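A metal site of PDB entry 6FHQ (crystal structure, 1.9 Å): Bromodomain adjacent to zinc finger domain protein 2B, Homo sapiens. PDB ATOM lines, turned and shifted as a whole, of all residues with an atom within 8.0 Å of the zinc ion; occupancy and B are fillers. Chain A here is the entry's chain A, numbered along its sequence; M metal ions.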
ATOM      1  N   TYR A   8       7.062  15.284 -24.712  1.00  0.00           N
ATOM      2  CA  TYR A   8       6.440  15.543 -23.438  1.00  0.00           C
ATOM      3  C   TYR A   8       6.377  17.090 -23.195  1.00  0.00           C
ATOM      4  O   TYR A   8       7.327  17.815 -23.522  1.00  0.00           O
ATOM      5  CB  TYR A   8       7.284  14.830 -22.343  1.00  0.00           C
ATOM      6  CG  TYR A   8       7.250  13.283 -22.431  1.00  0.00           C
ATOM      7  CD1 TYR A   8       6.242  12.548 -21.797  1.00  0.00           C
ATOM      8  CD2 TYR A   8       8.271  12.573 -23.077  1.00  0.00           C
ATOM      9  CE1 TYR A   8       6.192  11.203 -21.859  1.00  0.00           C
ATOM     10  CE2 TYR A   8       8.241  11.197 -23.146  1.00  0.00           C
ATOM     11  CZ  TYR A   8       7.169  10.509 -22.558  1.00  0.00           C
ATOM     12  OH  TYR A   8       7.063   9.143 -22.577  1.00  0.00           O
ATOM     13  N   CYS A   9       5.342  17.563 -22.502  1.00  0.00           N
ATOM     14  CA  CYS A   9       5.224  18.963 -22.183  1.00  0.00           C
ATOM     15  C   CYS A   9       6.351  19.402 -21.308  1.00  0.00           C
ATOM     16  O   CYS A   9       6.706  18.718 -20.345  1.00  0.00           O
ATOM     17  CB  CYS A   9       3.887  19.185 -21.437  1.00  0.00           C
ATOM     18  SG  CYS A   9       3.652  20.790 -20.731  1.00  0.00           S
ATOM     19  N   GLN A  10       6.978  20.493 -21.685  1.00  0.00           N
ATOM     20  CA  GLN A  10       8.149  21.048 -20.912  1.00  0.00           C
ATOM     21  C   GLN A  10       7.784  21.305 -19.456  1.00  0.00           C
ATOM     22  O   GLN A  10       8.636  21.186 -18.554  1.00  0.00           O
ATOM     23  CB  GLN A  10       8.610  22.349 -21.554  1.00  0.00           C
ATOM     24  CG  GLN A  10       9.358  22.133 -22.841  1.00  0.00           C
ATOM     25  CD  GLN A  10      10.695  21.440 -22.636  1.00  0.00           C
ATOM     26  OE1 GLN A  10      10.854  20.221 -22.939  1.00  0.00           O
ATOM     27  NE2 GLN A  10      11.692  22.205 -22.165  1.00  0.00           N
ATOM     28  N   ILE A  11       6.504  21.581 -19.207  1.00  0.00           N
ATOM     29  CA  ILE A  11       6.106  21.992 -17.914  1.00  0.00           C
ATOM     30  C   ILE A  11       5.624  20.841 -17.022  1.00  0.00           C
ATOM     31  O   ILE A  11       6.113  20.662 -15.918  1.00  0.00           O
ATOM     32  CB  ILE A  11       4.957  23.056 -18.004  1.00  0.00           C
ATOM     33  CG1 ILE A  11       5.463  24.323 -18.708  1.00  0.00           C
ATOM     34  CG2 ILE A  11       4.433  23.396 -16.572  1.00  0.00           C
ATOM     35  CD1 ILE A  11       6.702  24.908 -18.118  1.00  0.00           C
ATOM     36  N   CYS A  12       4.603  20.132 -17.428  1.00  0.00           N
ATOM     37  CA  CYS A  12       4.104  19.058 -16.618  1.00  0.00           C
ATOM     38  C   CYS A  12       4.807  17.716 -16.897  1.00  0.00           C
ATOM     39  O   CYS A  12       4.521  16.715 -16.211  1.00  0.00           O
ATOM     40  CB  CYS A  12       2.613  18.876 -16.812  1.00  0.00           C
ATOM     41  SG  CYS A  12       2.140  18.293 -18.437  1.00  0.00           S
ATOM     42  N   ARG A  13       5.650  17.665 -17.936  1.00  0.00           N
ATOM     43  CA  ARG A  13       6.313  16.415 -18.355  1.00  0.00           C
ATOM     44  C   ARG A  13       5.416  15.277 -18.728  1.00  0.00           C
ATOM     45  O   ARG A  13       5.871  14.148 -18.697  1.00  0.00           O
ATOM     46  CB  ARG A  13       7.273  15.903 -17.278  1.00  0.00           C
ATOM     47  CG  ARG A  13       8.112  16.954 -16.589  1.00  0.00           C
ATOM     48  CD  ARG A  13       8.730  17.930 -17.508  1.00  0.00           C
ATOM     49  NE  ARG A  13       9.876  17.377 -18.089  1.00  0.00           N
ATOM     50  CZ  ARG A  13      10.938  18.077 -18.463  1.00  0.00           C
ATOM     51  NH1 ARG A  13      10.895  19.401 -18.427  1.00  0.00           N
ATOM     52  NH2 ARG A  13      12.023  17.451 -18.920  1.00  0.00           N
ATOM     53  N   LYS A  14       4.173  15.532 -19.132  1.00  0.00           N
ATOM     54  CA  LYS A  14       3.322  14.458 -19.631  1.00  0.00           C
ATOM     55  C   LYS A  14       3.103  14.646 -21.121  1.00  0.00           C
ATOM     56  O   LYS A  14       3.211  15.765 -21.660  1.00  0.00           O
ATOM     57  CB  LYS A  14       1.954  14.437 -18.934  1.00  0.00           C
ATOM     58  CG  LYS A  14       2.012  14.465 -17.431  1.00  0.00           C
ATOM     59  CD  LYS A  14       0.645  14.921 -16.900  1.00  0.00           C
ATOM     60  CE  LYS A  14       0.426  14.641 -15.409  1.00  0.00           C
ATOM     61  NZ  LYS A  14      -0.926  14.023 -15.207  1.00  0.00           N
ATOM     62  N   GLY A  15       2.769  13.560 -21.805  1.00  0.00           N
ATOM     63  CA  GLY A  15       2.623  13.587 -23.278  1.00  0.00           C
ATOM     64  C   GLY A  15       1.221  13.343 -23.717  1.00  0.00           C
ATOM     65  O   GLY A  15       0.993  13.093 -24.875  1.00  0.00           O
ATOM     66  N   ASP A  16       0.278  13.394 -22.795  1.00  0.00           N
ATOM     67  CA  ASP A  16      -1.156  13.249 -23.124  1.00  0.00           C
ATOM     68  C   ASP A  16      -1.781  14.564 -23.658  1.00  0.00           C
ATOM     69  O   ASP A  16      -1.088  15.565 -23.813  1.00  0.00           O
ATOM     70  CB  ASP A  16      -1.913  12.807 -21.875  1.00  0.00           C
ATOM     71  CG  ASP A  16      -2.028  13.919 -20.827  1.00  0.00           C
ATOM     72  OD1 ASP A  16      -1.206  14.861 -20.839  1.00  0.00           O
ATOM     73  OD2 ASP A  16      -2.907  13.827 -19.952  1.00  0.00           O
ATOM     74  N   ASN A  17      -3.104  14.548 -23.895  1.00  0.00           N
ATOM     75  CA  ASN A  17      -3.848  15.675 -24.446  1.00  0.00           C
ATOM     76  C   ASN A  17      -3.096  16.254 -25.593  1.00  0.00           C
ATOM     77  O   ASN A  17      -2.759  17.414 -25.602  1.00  0.00           O
ATOM     78  CB  ASN A  17      -4.002  16.767 -23.411  1.00  0.00           C
ATOM     79  CG  ASN A  17      -5.285  16.674 -22.653  1.00  0.00           C
ATOM     80  OD1 ASN A  17      -6.346  16.421 -23.223  1.00  0.00           O
ATOM     81  ND2 ASN A  17      -5.209  16.943 -21.381  1.00  0.00           N
ATOM     82  N   LEU A  20      -3.689  19.500 -27.451  1.00  0.00           N
ATOM     83  CA  LEU A  20      -3.465  20.720 -26.740  1.00  0.00           C
ATOM     84  C   LEU A  20      -1.981  20.892 -26.497  1.00  0.00           C
ATOM     85  O   LEU A  20      -1.561  21.859 -25.884  1.00  0.00           O
ATOM     86  CB  LEU A  20      -4.239  20.692 -25.436  1.00  0.00           C
ATOM     87  CG  LEU A  20      -5.752  20.681 -25.565  1.00  0.00           C
ATOM     88  CD1 LEU A  20      -6.359  20.546 -24.181  1.00  0.00           C
ATOM     89  CD2 LEU A  20      -6.252  21.955 -26.267  1.00  0.00           C
ATOM     90  N   LEU A  21      -1.212  19.937 -26.993  1.00  0.00           N
ATOM     91  CA  LEU A  21       0.180  19.914 -26.729  1.00  0.00           C
ATOM     92  C   LEU A  21       0.880  20.621 -27.937  1.00  0.00           C
ATOM     93  O   LEU A  21       1.050  20.033 -29.022  1.00  0.00           O
ATOM     94  CB  LEU A  21       0.626  18.479 -26.535  1.00  0.00           C
ATOM     95  CG  LEU A  21       2.118  18.263 -26.353  1.00  0.00           C
ATOM     96  CD1 LEU A  21       2.681  19.042 -25.176  1.00  0.00           C
ATOM     97  CD2 LEU A  21       2.428  16.741 -26.264  1.00  0.00           C
ATOM     98  N   GLY A  30       7.633  20.791 -26.663  1.00  0.00           N
ATOM     99  CA  GLY A  30       6.187  20.840 -26.467  1.00  0.00           C
ATOM    100  C   GLY A  30       5.748  21.491 -25.184  1.00  0.00           C
ATOM    101  O   GLY A  30       6.471  21.545 -24.205  1.00  0.00           O
ATOM    102  N   CYS A  31       4.547  22.071 -25.205  1.00  0.00           N
ATOM    103  CA  CYS A  31       3.952  22.594 -24.003  1.00  0.00           C
ATOM    104  C   CYS A  31       2.470  22.676 -24.185  1.00  0.00           C
ATOM    105  O   CYS A  31       1.993  23.128 -25.234  1.00  0.00           O
ATOM    106  CB  CYS A  31       4.537  23.965 -23.694  1.00  0.00           C
ATOM    107  SG  CYS A  31       4.105  24.662 -22.087  1.00  0.00           S
ATOM    108  N   HIS A  32       1.708  22.173 -23.212  1.00  0.00           N
ATOM    109  CA  HIS A  32       0.268  22.213 -23.308  1.00  0.00           C
ATOM    110  C   HIS A  32      -0.210  23.695 -23.246  1.00  0.00           C
ATOM    111  O   HIS A  32       0.291  24.475 -22.417  1.00  0.00           O
ATOM    112  CB  HIS A  32      -0.383  21.489 -22.126  1.00  0.00           C
ATOM    113  CG  HIS A  32      -0.167  20.014 -22.113  1.00  0.00           C
ATOM    114  ND1 HIS A  32       0.621  19.378 -21.168  1.00  0.00           N
ATOM    115  CD2 HIS A  32      -0.663  19.038 -22.934  1.00  0.00           C
ATOM    116  CE1 HIS A  32       0.624  18.074 -21.442  1.00  0.00           C
ATOM    117  NE2 HIS A  32      -0.141  17.853 -22.501  1.00  0.00           N
ATOM    118  N   THR A  33      -1.326  23.974 -23.935  1.00  0.00           N
ATOM    119  CA  THR A  33      -1.982  25.270 -23.825  1.00  0.00           C
ATOM    120  C   THR A  33      -2.169  25.723 -22.359  1.00  0.00           C
ATOM    121  O   THR A  33      -1.808  26.852 -21.961  1.00  0.00           O
ATOM    122  CB  THR A  33      -3.391  25.215 -24.437  1.00  0.00           C
ATOM    123  OG1 THR A  33      -4.053  24.020 -24.022  1.00  0.00           O
ATOM    124  CG2 THR A  33      -3.337  25.254 -25.918  1.00  0.00           C
ATOM    125  N   TYR A  34      -2.730  24.807 -21.580  1.00  0.00           N
ATOM    126  CA  TYR A  34      -3.108  25.042 -20.219  1.00  0.00           C
ATOM    127  C   TYR A  34      -1.955  24.955 -19.250  1.00  0.00           C
ATOM    128  O   TYR A  34      -2.130  25.374 -18.149  1.00  0.00           O
ATOM    129  CB  TYR A  34      -4.204  24.058 -19.782  1.00  0.00           C
ATOM    130  CG  TYR A  34      -3.887  22.610 -19.972  1.00  0.00           C
ATOM    131  CD1 TYR A  34      -3.049  21.953 -19.087  1.00  0.00           C
ATOM    132  CD2 TYR A  34      -4.349  21.933 -21.061  1.00  0.00           C
ATOM    133  CE1 TYR A  34      -2.737  20.661 -19.216  1.00  0.00           C
ATOM    134  CE2 TYR A  34      -4.061  20.607 -21.209  1.00  0.00           C
ATOM    135  CZ  TYR A  34      -3.220  19.966 -20.273  1.00  0.00           C
ATOM    136  OH  TYR A  34      -2.792  18.632 -20.451  1.00  0.00           O
ATOM    137  N   CYS A  35      -0.772  24.540 -19.690  1.00  0.00           N
ATOM    138  CA  CYS A  35       0.462  24.656 -18.848  1.00  0.00           C
ATOM    139  C   CYS A  35       1.283  25.941 -18.986  1.00  0.00           C
ATOM    140  O   CYS A  35       2.009  26.313 -18.048  1.00  0.00           O
ATOM    141  CB  CYS A  35       1.414  23.453 -19.080  1.00  0.00           C
ATOM    142  SG  CYS A  35       0.694  21.900 -18.538  1.00  0.00           S
ATOM    143  N   HIS A  36       1.159  26.635 -20.118  1.00  0.00           N
ATOM    144  CA  HIS A  36       1.633  27.979 -20.214  1.00  0.00           C
ATOM    145  C   HIS A  36       0.988  28.908 -19.174  1.00  0.00           C
ATOM    146  O   HIS A  36      -0.153  28.681 -18.761  1.00  0.00           O
ATOM    147  CB  HIS A  36       1.252  28.596 -21.520  1.00  0.00           C
ATOM    148  CG  HIS A  36       2.026  28.076 -22.640  1.00  0.00           C
ATOM    149  ND1 HIS A  36       3.295  28.506 -22.920  1.00  0.00           N
ATOM    150  CD2 HIS A  36       1.720  27.149 -23.560  1.00  0.00           C
ATOM    151  CE1 HIS A  36       3.717  27.919 -24.030  1.00  0.00           C
ATOM    152  NE2 HIS A  36       2.797  27.067 -24.414  1.00  0.00           N
HETATM  153 ZN    ZN M   1       1.687  20.187 -19.726  1.00  0.00          ZN
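A ring nitrogen (NE2) of His 32 lies close to the side-chain hydroxyl of Tyr 34.
O of Asp 16 is in hydrogen-bond range of NE2 of His 32 (2.8 Å).
The backbone NH of Ile 11 sits close to the side-chain sulfur of Cys 9 (3.3 Å).
The backbone carbonyl oxygen (O) of Lys 14 is in hydrogen-bond range of the backbone NH (N) of Cys 9 (2.9 Å).
The side-chain sulfur (SG) of Cys 12 sits close to the backbone NH (N) of Lys 14 (3.5 Å).
Of the 19 residues printed, 4 come within 4 Å of the zinc ion.
The nearest printed residue that does not touch the zinc ion is Tyr 34 (4.5 Å).
The zinc ion is bound by a ring nitrogen (ND1) of His 32 (2.0 Å), the side-chain sulfur of Cys 9 (2.3 Å), the side-chain sulfur of Cys 35 (2.3 Å) and the side-chain sulfur of Cys 12 (2.3 Å).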
